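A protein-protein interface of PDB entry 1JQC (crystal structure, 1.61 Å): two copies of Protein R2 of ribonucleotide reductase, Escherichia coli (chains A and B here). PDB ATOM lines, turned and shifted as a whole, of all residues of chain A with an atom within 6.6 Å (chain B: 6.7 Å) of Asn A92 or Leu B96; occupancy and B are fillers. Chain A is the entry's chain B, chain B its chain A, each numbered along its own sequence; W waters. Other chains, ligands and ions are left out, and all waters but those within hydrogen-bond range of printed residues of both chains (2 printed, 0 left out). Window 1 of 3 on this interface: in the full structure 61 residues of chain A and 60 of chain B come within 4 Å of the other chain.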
ATOM      1  N   GLN A  87      -1.492 -12.675 -12.541  1.00  0.00           N
ATOM      2  CA  GLN A  87      -2.461 -12.265 -13.561  1.00  0.00           C
ATOM      3  C   GLN A  87      -2.315 -12.957 -14.884  1.00  0.00           C
ATOM      4  O   GLN A  87      -3.230 -12.936 -15.662  1.00  0.00           O
ATOM      5  CB  GLN A  87      -2.393 -10.757 -13.741  1.00  0.00           C
ATOM      6  CG  GLN A  87      -2.973  -9.968 -12.549  1.00  0.00           C
ATOM      7  CD  GLN A  87      -4.429 -10.162 -12.468  1.00  0.00           C
ATOM      8  OE1 GLN A  87      -5.223  -9.552 -13.218  1.00  0.00           O
ATOM      9  NE2 GLN A  87      -4.808 -11.005 -11.597  1.00  0.00           N
ATOM     10  N   GLY A  88      -1.179 -13.604 -15.141  1.00  0.00           N
ATOM     11  CA  GLY A  88      -1.115 -14.309 -16.411  1.00  0.00           C
ATOM     12  C   GLY A  88      -1.968 -15.576 -16.363  1.00  0.00           C
ATOM     13  O   GLY A  88      -2.613 -15.947 -17.333  1.00  0.00           O
ATOM     14  N   ARG A  89      -1.997 -16.261 -15.204  1.00  0.00           N
ATOM     15  CA  ARG A  89      -2.754 -17.518 -15.128  1.00  0.00           C
ATOM     16  C   ARG A  89      -4.137 -17.369 -14.551  1.00  0.00           C
ATOM     17  O   ARG A  89      -5.033 -18.051 -14.984  1.00  0.00           O
ATOM     18  CB  ARG A  89      -2.010 -18.586 -14.238  1.00  0.00           C
ATOM     19  CG  ARG A  89      -1.900 -18.174 -12.719  1.00  0.00           C
ATOM     20  CD  ARG A  89      -1.029 -19.259 -11.978  1.00  0.00           C
ATOM     21  NE  ARG A  89       0.343 -19.207 -12.484  1.00  0.00           N
ATOM     22  CZ  ARG A  89       1.354 -18.585 -11.902  1.00  0.00           C
ATOM     23  NH1 ARG A  89       1.231 -17.944 -10.716  1.00  0.00           N
ATOM     24  NH2 ARG A  89       2.499 -18.554 -12.545  1.00  0.00           N
ATOM     25  N   SER A  90      -4.312 -16.439 -13.613  1.00  0.00           N
ATOM     26  CA  SER A  90      -5.565 -16.457 -12.855  1.00  0.00           C
ATOM     27  C   SER A  90      -6.844 -16.104 -13.559  1.00  0.00           C
ATOM     28  O   SER A  90      -7.867 -16.746 -13.347  1.00  0.00           O
ATOM     29  CB  SER A  90      -5.377 -15.694 -11.514  1.00  0.00           C
ATOM     30  OG  SER A  90      -4.244 -16.209 -10.823  1.00  0.00           O
ATOM     31  N   PRO A  91      -6.845 -15.092 -14.416  1.00  0.00           N
ATOM     32  CA  PRO A  91      -8.106 -14.805 -15.099  1.00  0.00           C
ATOM     33  C   PRO A  91      -8.555 -16.057 -15.888  1.00  0.00           C
ATOM     34  O   PRO A  91      -9.725 -16.389 -15.950  1.00  0.00           O
ATOM     35  CB  PRO A  91      -7.713 -13.641 -16.028  1.00  0.00           C
ATOM     36  CG  PRO A  91      -6.657 -12.929 -15.278  1.00  0.00           C
ATOM     37  CD  PRO A  91      -5.806 -14.116 -14.754  1.00  0.00           C
ATOM     38  N   ASN A  92      -7.614 -16.785 -16.486  1.00  0.00           N
ATOM     39  CA  ASN A  92      -7.969 -17.979 -17.224  1.00  0.00           C
ATOM     40  C   ASN A  92      -8.478 -19.129 -16.335  1.00  0.00           C
ATOM     41  O   ASN A  92      -9.565 -19.640 -16.589  1.00  0.00           O
ATOM     42  CB  ASN A  92      -6.783 -18.535 -18.060  1.00  0.00           C
ATOM     43  CG  ASN A  92      -6.546 -17.766 -19.349  1.00  0.00           C
ATOM     44  OD1 ASN A  92      -7.470 -17.193 -19.933  1.00  0.00           O
ATOM     45  ND2 ASN A  92      -5.316 -17.742 -19.788  1.00  0.00           N
ATOM     46  N   VAL A  93      -7.758 -19.427 -15.238  1.00  0.00           N
ATOM     47  CA  VAL A  93      -8.173 -20.561 -14.433  1.00  0.00           C
ATOM     48  C   VAL A  93      -9.421 -20.256 -13.621  1.00  0.00           C
ATOM     49  O   VAL A  93     -10.212 -21.174 -13.376  1.00  0.00           O
ATOM     50  CB  VAL A  93      -7.032 -21.030 -13.498  1.00  0.00           C
ATOM     51  CG1 VAL A  93      -7.540 -22.070 -12.506  1.00  0.00           C
ATOM     52  CG2 VAL A  93      -5.906 -21.674 -14.355  1.00  0.00           C
ATOM     53  N   ALA A  94      -9.578 -18.986 -13.192  1.00  0.00           N
ATOM     54  CA  ALA A  94     -10.732 -18.587 -12.355  1.00  0.00           C
ATOM     55  C   ALA A  94     -11.961 -18.119 -13.088  1.00  0.00           C
ATOM     56  O   ALA A  94     -13.087 -18.405 -12.676  1.00  0.00           O
ATOM     57  CB  ALA A  94     -10.299 -17.464 -11.377  1.00  0.00           C
ATOM     58  N   LEU A  95     -11.780 -17.396 -14.195  1.00  0.00           N
ATOM     59  CA  LEU A  95     -12.966 -16.889 -14.876  1.00  0.00           C
ATOM     60  C   LEU A  95     -13.434 -17.666 -16.050  1.00  0.00           C
ATOM     61  O   LEU A  95     -14.650 -17.793 -16.257  1.00  0.00           O
ATOM     62  CB  LEU A  95     -12.718 -15.429 -15.298  1.00  0.00           C
ATOM     63  CG  LEU A  95     -12.194 -14.545 -14.166  1.00  0.00           C
ATOM     64  CD1 LEU A  95     -11.950 -13.143 -14.747  1.00  0.00           C
ATOM     65  CD2 LEU A  95     -13.215 -14.418 -13.015  1.00  0.00           C
ATOM     66  N   LEU A  96     -12.521 -18.215 -16.873  1.00  0.00           N
ATOM     67  CA  LEU A  96     -13.032 -18.975 -18.035  1.00  0.00           C
ATOM     68  C   LEU A  96     -14.068 -20.042 -17.763  1.00  0.00           C
ATOM     69  O   LEU A  96     -15.038 -20.192 -18.521  1.00  0.00           O
ATOM     70  CB  LEU A  96     -11.927 -19.697 -18.846  1.00  0.00           C
ATOM     71  CG  LEU A  96     -10.980 -18.824 -19.537  1.00  0.00           C
ATOM     72  CD1 LEU A  96      -9.925 -19.690 -20.210  1.00  0.00           C
ATOM     73  CD2 LEU A  96     -11.829 -18.007 -20.613  1.00  0.00           C
ATOM     74  N   PRO A  97     -13.941 -20.793 -16.644  1.00  0.00           N
ATOM     75  CA  PRO A  97     -14.943 -21.831 -16.440  1.00  0.00           C
ATOM     76  C   PRO A  97     -16.331 -21.285 -16.117  1.00  0.00           C
ATOM     77  O   PRO A  97     -17.298 -22.024 -16.107  1.00  0.00           O
ATOM     78  CB  PRO A  97     -14.349 -22.653 -15.245  1.00  0.00           C
ATOM     79  CG  PRO A  97     -12.840 -22.405 -15.350  1.00  0.00           C
ATOM     80  CD  PRO A  97     -12.750 -20.924 -15.766  1.00  0.00           C
ATOM     81  N   GLU A 105     -15.318 -14.217 -22.983  1.00  0.00           N
ATOM     82  CA  GLU A 105     -14.386 -15.333 -22.905  1.00  0.00           C
ATOM     83  C   GLU A 105     -13.107 -14.980 -23.639  1.00  0.00           C
ATOM     84  O   GLU A 105     -12.007 -15.157 -23.110  1.00  0.00           O
ATOM     85  CB  GLU A 105     -15.024 -16.581 -23.548  1.00  0.00           C
ATOM     86  CG  GLU A 105     -14.141 -17.836 -23.398  1.00  0.00           C
ATOM     87  CD  GLU A 105     -14.651 -19.003 -24.212  1.00  0.00           C
ATOM     88  OE1 GLU A 105     -14.649 -18.940 -25.443  1.00  0.00           O
ATOM     89  OE2 GLU A 105     -15.014 -20.010 -23.612  1.00  0.00           O
ATOM     90  N   VAL A 108     -11.062 -12.295 -21.777  1.00  0.00           N
ATOM     91  CA  VAL A 108     -10.250 -12.827 -20.691  1.00  0.00           C
ATOM     92  C   VAL A 108      -9.006 -13.539 -21.159  1.00  0.00           C
ATOM     93  O   VAL A 108      -7.915 -13.332 -20.564  1.00  0.00           O
ATOM     94  CB  VAL A 108     -11.097 -13.745 -19.806  1.00  0.00           C
ATOM     95  CG1 VAL A 108     -10.230 -14.549 -18.849  1.00  0.00           C
ATOM     96  CG2 VAL A 108     -12.061 -12.876 -19.021  1.00  0.00           C
ATOM     97  N   GLU A 109      -9.120 -14.357 -22.215  1.00  0.00           N
ATOM     98  CA  GLU A 109      -7.905 -15.028 -22.709  1.00  0.00           C
ATOM     99  C   GLU A 109      -6.908 -14.035 -23.303  1.00  0.00           C
ATOM    100  O   GLU A 109      -5.704 -14.245 -23.225  1.00  0.00           O
ATOM    101  CB  GLU A 109      -8.275 -16.083 -23.757  1.00  0.00           C
ATOM    102  CG  GLU A 109      -9.229 -17.155 -23.122  1.00  0.00           C
ATOM    103  CD  GLU A 109      -9.350 -18.382 -23.930  1.00  0.00           C
ATOM    104  OE1 GLU A 109      -8.432 -19.255 -23.882  1.00  0.00           O
ATOM    105  OE2 GLU A 109     -10.371 -18.479 -24.618  1.00  0.00           O
ATOM    106  N   THR A 110      -7.397 -12.933 -23.887  1.00  0.00           N
ATOM    107  CA  THR A 110      -6.506 -11.922 -24.475  1.00  0.00           C
ATOM    108  C   THR A 110      -5.814 -11.109 -23.393  1.00  0.00           C
ATOM    109  O   THR A 110      -4.622 -10.866 -23.464  1.00  0.00           O
ATOM    110  CB  THR A 110      -7.326 -11.025 -25.412  1.00  0.00           C
ATOM    111  OG1 THR A 110      -7.878 -11.851 -26.453  1.00  0.00           O
ATOM    112  CG2 THR A 110      -6.472  -9.929 -26.042  1.00  0.00           C
ATOM    113  N   ALA A 112      -5.305 -12.136 -20.249  1.00  0.00           N
ATOM    114  CA  ALA A 112      -4.336 -13.000 -19.571  1.00  0.00           C
ATOM    115  C   ALA A 112      -3.070 -13.146 -20.412  1.00  0.00           C
ATOM    116  O   ALA A 112      -1.948 -13.085 -19.880  1.00  0.00           O
ATOM    117  CB  ALA A 112      -4.957 -14.359 -19.298  1.00  0.00           C
ATOM    118  N   PHE A 113      -3.221 -13.294 -21.747  1.00  0.00           N
ATOM    119  CA  PHE A 113      -2.056 -13.406 -22.592  1.00  0.00           C
ATOM    120  C   PHE A 113      -1.180 -12.150 -22.496  1.00  0.00           C
ATOM    121  O   PHE A 113       0.042 -12.241 -22.415  1.00  0.00           O
ATOM    122  CB  PHE A 113      -2.527 -13.585 -24.031  1.00  0.00           C
ATOM    123  CG  PHE A 113      -1.438 -13.385 -25.042  1.00  0.00           C
ATOM    124  CD1 PHE A 113      -0.387 -14.295 -25.147  1.00  0.00           C
ATOM    125  CD2 PHE A 113      -1.437 -12.239 -25.815  1.00  0.00           C
ATOM    126  CE1 PHE A 113       0.662 -14.044 -26.026  1.00  0.00           C
ATOM    127  CE2 PHE A 113      -0.403 -11.968 -26.702  1.00  0.00           C
ATOM    128  CZ  PHE A 113       0.654 -12.884 -26.801  1.00  0.00           C
ATOM    129  N   TYR B   2      -5.620 -26.522  -5.473  1.00  0.00           N
ATOM    130  CA  TYR B   2      -4.927 -25.775  -6.497  1.00  0.00           C
ATOM    131  C   TYR B   2      -4.708 -24.369  -5.931  1.00  0.00           C
ATOM    132  O   TYR B   2      -5.532 -23.855  -5.146  1.00  0.00           O
ATOM    133  CB  TYR B   2      -5.775 -25.673  -7.762  1.00  0.00           C
ATOM    134  CG  TYR B   2      -5.184 -24.732  -8.783  1.00  0.00           C
ATOM    135  CD1 TYR B   2      -4.148 -25.153  -9.619  1.00  0.00           C
ATOM    136  CD2 TYR B   2      -5.609 -23.414  -8.880  1.00  0.00           C
ATOM    137  CE1 TYR B   2      -3.552 -24.312 -10.492  1.00  0.00           C
ATOM    138  CE2 TYR B   2      -5.015 -22.559  -9.775  1.00  0.00           C
ATOM    139  CZ  TYR B   2      -3.992 -22.996 -10.571  1.00  0.00           C
ATOM    140  OH  TYR B   2      -3.385 -22.158 -11.451  1.00  0.00           O
ATOM    141  N   PHE B  18       3.935 -31.755 -15.623  1.00  0.00           N
ATOM    142  CA  PHE B  18       2.598 -31.795 -15.060  1.00  0.00           C
ATOM    143  C   PHE B  18       2.555 -32.457 -13.692  1.00  0.00           C
ATOM    144  O   PHE B  18       3.383 -33.287 -13.354  1.00  0.00           O
ATOM    145  CB  PHE B  18       1.686 -32.610 -15.984  1.00  0.00           C
ATOM    146  CG  PHE B  18       1.575 -32.064 -17.393  1.00  0.00           C
ATOM    147  CD1 PHE B  18       0.658 -31.048 -17.699  1.00  0.00           C
ATOM    148  CD2 PHE B  18       2.379 -32.577 -18.411  1.00  0.00           C
ATOM    149  CE1 PHE B  18       0.533 -30.550 -19.002  1.00  0.00           C
ATOM    150  CE2 PHE B  18       2.251 -32.077 -19.723  1.00  0.00           C
ATOM    151  CZ  PHE B  18       1.337 -31.072 -20.018  1.00  0.00           C
ATOM    152  N   SER B  90      -9.843 -24.681 -24.432  1.00  0.00           N
ATOM    153  CA  SER B  90      -9.532 -25.950 -23.763  1.00  0.00           C
ATOM    154  C   SER B  90      -8.130 -26.121 -23.187  1.00  0.00           C
ATOM    155  O   SER B  90      -8.002 -26.655 -22.087  1.00  0.00           O
ATOM    156  CB  SER B  90      -9.966 -27.160 -24.648  1.00  0.00           C
ATOM    157  OG  SER B  90     -11.395 -27.094 -24.880  1.00  0.00           O
ATOM    158  N   PRO B  91      -7.091 -25.670 -23.880  1.00  0.00           N
ATOM    159  CA  PRO B  91      -5.760 -25.837 -23.283  1.00  0.00           C
ATOM    160  C   PRO B  91      -5.702 -25.064 -21.955  1.00  0.00           C
ATOM    161  O   PRO B  91      -5.103 -25.520 -20.981  1.00  0.00           O
ATOM    162  CB  PRO B  91      -4.809 -25.241 -24.353  1.00  0.00           C
ATOM    163  CG  PRO B  91      -5.567 -25.635 -25.670  1.00  0.00           C
ATOM    164  CD  PRO B  91      -7.003 -25.248 -25.306  1.00  0.00           C
ATOM    165  N   ASN B  92      -6.380 -23.912 -21.888  1.00  0.00           N
ATOM    166  CA  ASN B  92      -6.372 -23.113 -20.679  1.00  0.00           C
ATOM    167  C   ASN B  92      -7.240 -23.727 -19.583  1.00  0.00           C
ATOM    168  O   ASN B  92      -6.843 -23.698 -18.438  1.00  0.00           O
ATOM    169  CB  ASN B  92      -6.870 -21.693 -20.953  1.00  0.00           C
ATOM    170  CG  ASN B  92      -5.782 -20.802 -21.548  1.00  0.00           C
ATOM    171  OD1 ASN B  92      -4.589 -20.985 -21.293  1.00  0.00           O
ATOM    172  ND2 ASN B  92      -6.199 -19.787 -22.276  1.00  0.00           N
ATOM    173  N   VAL B  93      -8.414 -24.267 -19.894  1.00  0.00           N
ATOM    174  CA  VAL B  93      -9.182 -24.850 -18.808  1.00  0.00           C
ATOM    175  C   VAL B  93      -8.761 -26.244 -18.385  1.00  0.00           C
ATOM    176  O   VAL B  93      -8.937 -26.621 -17.215  1.00  0.00           O
ATOM    177  CB  VAL B  93     -10.657 -24.832 -19.211  1.00  0.00           C
ATOM    178  CG1 VAL B  93     -11.501 -25.572 -18.182  1.00  0.00           C
ATOM    179  CG2 VAL B  93     -11.080 -23.344 -19.356  1.00  0.00           C
ATOM    180  N   ALA B  94      -8.203 -27.009 -19.310  1.00  0.00           N
ATOM    181  CA  ALA B  94      -7.838 -28.381 -19.025  1.00  0.00           C
ATOM    182  C   ALA B  94      -6.372 -28.618 -18.704  1.00  0.00           C
ATOM    183  O   ALA B  94      -6.054 -29.486 -17.880  1.00  0.00           O
ATOM    184  CB  ALA B  94      -8.320 -29.295 -20.223  1.00  0.00           C
ATOM    185  N   LEU B  95      -5.462 -27.860 -19.311  1.00  0.00           N
ATOM    186  CA  LEU B  95      -4.068 -28.090 -19.057  1.00  0.00           C
ATOM    187  C   LEU B  95      -3.447 -27.168 -18.077  1.00  0.00           C
ATOM    188  O   LEU B  95      -2.697 -27.595 -17.247  1.00  0.00           O
ATOM    189  CB  LEU B  95      -3.281 -28.080 -20.415  1.00  0.00           C
ATOM    190  CG  LEU B  95      -3.903 -28.963 -21.490  1.00  0.00           C
ATOM    191  CD1 LEU B  95      -3.031 -28.871 -22.790  1.00  0.00           C
ATOM    192  CD2 LEU B  95      -3.929 -30.446 -21.030  1.00  0.00           C
ATOM    193  N   LEU B  96      -3.789 -25.862 -18.122  1.00  0.00           N
ATOM    194  CA  LEU B  96      -3.196 -24.892 -17.226  1.00  0.00           C
ATOM    195  C   LEU B  96      -3.230 -25.259 -15.745  1.00  0.00           C
ATOM    196  O   LEU B  96      -2.243 -25.117 -15.021  1.00  0.00           O
ATOM    197  CB  LEU B  96      -3.877 -23.525 -17.418  1.00  0.00           C
ATOM    198  CG  LEU B  96      -3.164 -22.330 -17.950  1.00  0.00           C
ATOM    199  CD1 LEU B  96      -4.086 -21.129 -17.740  1.00  0.00           C
ATOM    200  CD2 LEU B  96      -1.823 -22.132 -17.259  1.00  0.00           C
ATOM    201  N   PRO B  97      -4.344 -25.829 -15.269  1.00  0.00           N
ATOM    202  CA  PRO B  97      -4.372 -26.159 -13.846  1.00  0.00           C
ATOM    203  C   PRO B  97      -3.402 -27.281 -13.420  1.00  0.00           C
ATOM    204  O   PRO B  97      -3.159 -27.475 -12.228  1.00  0.00           O
ATOM    205  CB  PRO B  97      -5.847 -26.584 -13.612  1.00  0.00           C
ATOM    206  CG  PRO B  97      -6.601 -25.738 -14.637  1.00  0.00           C
ATOM    207  CD  PRO B  97      -5.692 -25.905 -15.880  1.00  0.00           C
ATOM    208  N   LEU B  98      -2.842 -28.004 -14.384  1.00  0.00           N
ATOM    209  CA  LEU B  98      -1.964 -29.130 -14.068  1.00  0.00           C
ATOM    210  C   LEU B  98      -0.479 -28.911 -14.375  1.00  0.00           C
ATOM    211  O   LEU B  98       0.352 -29.791 -14.127  1.00  0.00           O
ATOM    212  CB  LEU B  98      -2.401 -30.354 -14.874  1.00  0.00           C
ATOM    213  CG  LEU B  98      -3.843 -30.821 -14.635  1.00  0.00           C
ATOM    214  CD1 LEU B  98      -4.229 -31.948 -15.636  1.00  0.00           C
ATOM    215  CD2 LEU B  98      -3.921 -31.293 -13.148  1.00  0.00           C
ATOM    216  N   ILE B  99      -0.127 -27.731 -14.904  1.00  0.00           N
ATOM    217  CA  ILE B  99       1.254 -27.466 -15.272  1.00  0.00           C
ATOM    218  C   ILE B  99       2.103 -26.984 -14.118  1.00  0.00           C
ATOM    219  O   ILE B  99       1.690 -26.139 -13.345  1.00  0.00           O
ATOM    220  CB  ILE B  99       1.300 -26.423 -16.430  1.00  0.00           C
ATOM    221  CG1 ILE B  99       0.620 -27.062 -17.629  1.00  0.00           C
ATOM    222  CG2 ILE B  99       2.778 -25.968 -16.751  1.00  0.00           C
ATOM    223  CD1 ILE B  99       0.383 -26.028 -18.733  1.00  0.00           C
ATOM    224  N   SER B 100       3.323 -27.517 -14.056  1.00  0.00           N
ATOM    225  CA  SER B 100       4.249 -27.163 -12.999  1.00  0.00           C
ATOM    226  C   SER B 100       5.606 -26.574 -13.373  1.00  0.00           C
ATOM    227  O   SER B 100       6.475 -26.429 -12.499  1.00  0.00           O
ATOM    228  CB  SER B 100       4.420 -28.376 -11.985  1.00  0.00           C
ATOM    229  OG  SER B 100       4.439 -29.636 -12.675  1.00  0.00           O
ATOM    230  N   LEU B 104       6.303 -24.067 -19.846  1.00  0.00           N
ATOM    231  CA  LEU B 104       5.151 -24.789 -20.429  1.00  0.00           C
ATOM    232  C   LEU B 104       3.849 -24.072 -20.077  1.00  0.00           C
ATOM    233  O   LEU B 104       2.945 -24.027 -20.921  1.00  0.00           O
ATOM    234  CB  LEU B 104       5.161 -26.253 -19.930  1.00  0.00           C
ATOM    235  CG  LEU B 104       4.015 -27.091 -20.395  1.00  0.00           C
ATOM    236  CD1 LEU B 104       4.001 -27.185 -21.933  1.00  0.00           C
ATOM    237  CD2 LEU B 104       4.132 -28.508 -19.787  1.00  0.00           C
ATOM    238  N   GLU B 105       3.762 -23.455 -18.891  1.00  0.00           N
ATOM    239  CA  GLU B 105       2.535 -22.734 -18.557  1.00  0.00           C
ATOM    240  C   GLU B 105       2.320 -21.580 -19.583  1.00  0.00           C
ATOM    241  O   GLU B 105       1.223 -21.440 -20.155  1.00  0.00           O
ATOM    242  CB  GLU B 105       2.658 -22.174 -17.138  1.00  0.00           C
ATOM    243  CG  GLU B 105       1.394 -21.403 -16.708  1.00  0.00           C
ATOM    244  CD  GLU B 105       1.608 -20.629 -15.395  1.00  0.00           C
ATOM    245  OE1 GLU B 105       2.316 -19.610 -15.410  1.00  0.00           O
ATOM    246  OE2 GLU B 105       1.028 -21.079 -14.391  1.00  0.00           O
ATOM    247  N   THR B 106       3.353 -20.802 -19.820  1.00  0.00           N
ATOM    248  CA  THR B 106       3.198 -19.682 -20.764  1.00  0.00           C
ATOM    249  C   THR B 106       3.035 -20.163 -22.200  1.00  0.00           C
ATOM    250  O   THR B 106       2.296 -19.535 -22.974  1.00  0.00           O
ATOM    251  CB  THR B 106       4.352 -18.724 -20.571  1.00  0.00           C
ATOM    252  OG1 THR B 106       4.303 -18.207 -19.211  1.00  0.00           O
ATOM    253  CG2 THR B 106       4.267 -17.563 -21.562  1.00  0.00           C
ATOM    254  N   VAL B 108       1.382 -22.855 -23.086  1.00  0.00           N
ATOM    255  CA  VAL B 108      -0.007 -23.193 -23.208  1.00  0.00           C
ATOM    256  C   VAL B 108      -0.906 -21.961 -23.323  1.00  0.00           C
ATOM    257  O   VAL B 108      -1.825 -21.977 -24.160  1.00  0.00           O
ATOM    258  CB  VAL B 108      -0.426 -24.102 -22.011  1.00  0.00           C
ATOM    259  CG1 VAL B 108      -1.946 -24.209 -21.948  1.00  0.00           C
ATOM    260  CG2 VAL B 108       0.183 -25.484 -22.245  1.00  0.00           C
ATOM    261  N   GLU B 109      -0.636 -20.894 -22.557  1.00  0.00           N
ATOM    262  CA  GLU B 109      -1.482 -19.717 -22.651  1.00  0.00           C
ATOM    263  C   GLU B 109      -1.264 -19.001 -23.984  1.00  0.00           C
ATOM    264  O   GLU B 109      -2.199 -18.348 -24.509  1.00  0.00           O
ATOM    265  CB  GLU B 109      -1.209 -18.755 -21.492  1.00  0.00           C
ATOM    266  CG  GLU B 109      -1.472 -19.436 -20.150  1.00  0.00           C
ATOM    267  CD  GLU B 109      -1.518 -18.462 -19.018  1.00  0.00           C
ATOM    268  OE1 GLU B 109      -0.531 -18.366 -18.283  1.00  0.00           O
ATOM    269  OE2 GLU B 109      -2.566 -17.783 -18.857  1.00  0.00           O
ATOM    270  N   ALA B 112      -3.071 -21.216 -26.675  1.00  0.00           N
ATOM    271  CA  ALA B 112      -4.550 -20.990 -26.606  1.00  0.00           C
ATOM    272  C   ALA B 112      -4.891 -19.613 -27.167  1.00  0.00           C
ATOM    273  O   ALA B 112      -5.863 -19.486 -27.914  1.00  0.00           O
ATOM    274  CB  ALA B 112      -5.040 -21.096 -25.150  1.00  0.00           C
HETATM  275  O   HOH W   1       1.578 -16.526 -15.182  1.00  0.00           O
HETATM  276  O   HOH W   2      -4.436 -16.936 -22.746  1.00  0.00           O
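The backbone NH (N) of Leu B96 lies within hydrogen-bond range of the backbone carbonyl oxygen (O) of Pro B91, 3.2 Å away. The backbone carbonyl oxygen (O) of Pro A91 is in hydrogen-bond range of the backbone NH (N) of Leu A96.
Of chain B, only Asn B92 (3.3 Å), Leu B96 (3.8 Å) and Glu B109 (2.9 Å) come within 4 Å of Asn A92. Leu B96 touches just these residues of chain A: Asn A92 and Val A93. Printed residues of chain B within 4 Å of Glu A109: Asn B92. Printed residues of chain A within 4 Å of Val B93: Leu A96. Of the printed residues of chain A, Asn B92 touches Asn A92, Leu A96 and Glu A109. Of the printed residues of chain A, Glu B105 touches Arg A89. Printed residues of chain B within 4 Å of Val A93: Tyr B2 (3.8 Å) and Leu B96 (3.9 Å).
Arg A89 touches Tyr B2 (CD to OH, 3.8 Å). CA of Arg A89 touches OE2 of Glu B109, at 3.7 Å. Asn A92 touches Leu B96. Tyr B2 touches Val A93. Val A93 touches Leu B96 (CG2 to CD1, 3.9 Å). Asn B92 touches Leu A96. CG2 of Val B93 touches CB of Leu A96, at 3.8 Å.
Hydrophobic or aromatic side chains of chain A that line the printed part of chain B: Val A93 and Leu A96. Among the printed residues, 12 pairs touch across the chains. Among the printed residues, Asp or Glu carboxylates within 4 Å of a Lys or Arg side-chain nitrogen of the other chain: Arg A89 with Glu B105.
Water W2 lies within hydrogen-bond range of O of Glu A109, O of Glu B109, ND2 of Asn A92 and ND2 of Asn B92. Water W1 lies within hydrogen-bond range of OE1 of Glu B105 (3.2 Å) and NH2 of Arg A89 (3.5 Å).
The side-chain amide nitrogen of Asn B92 sits close to the side-chain amide nitrogen of Asn A92 (3.3 Å). ND2 of Asn B92 sits at hydrogen-bond distance from OE1 of Glu A109, at 2.8 Å. NE of Arg A89 is in salt-bridge range of OE2 of Glu B105, at 2.8 Å. The side-chain amide nitrogen of Asn A92 lies within hydrogen-bond range of the side-chain carboxylate of Glu B109 (2.9 Å). The side-chain carboxylate (OE2) of Glu B109 sits close to the backbone carbonyl oxygen (O) of Gly A88 (2.4 Å).
Asn A92 touches its own counterpart, Asn B92. Asn A92 touches Leu B96, and with the chains exchanged Leu A96 touches Asn B92. Asn A92 touches Glu B109, and with the chains exchanged Glu A109 touches Asn B92. Val A93 touches Leu B96, and with the chains exchanged Leu A96 touches Val B93. Of the 12 pairs that touch across the chains among the printed residues, 7 have their exchanged pair printed and touching as well.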
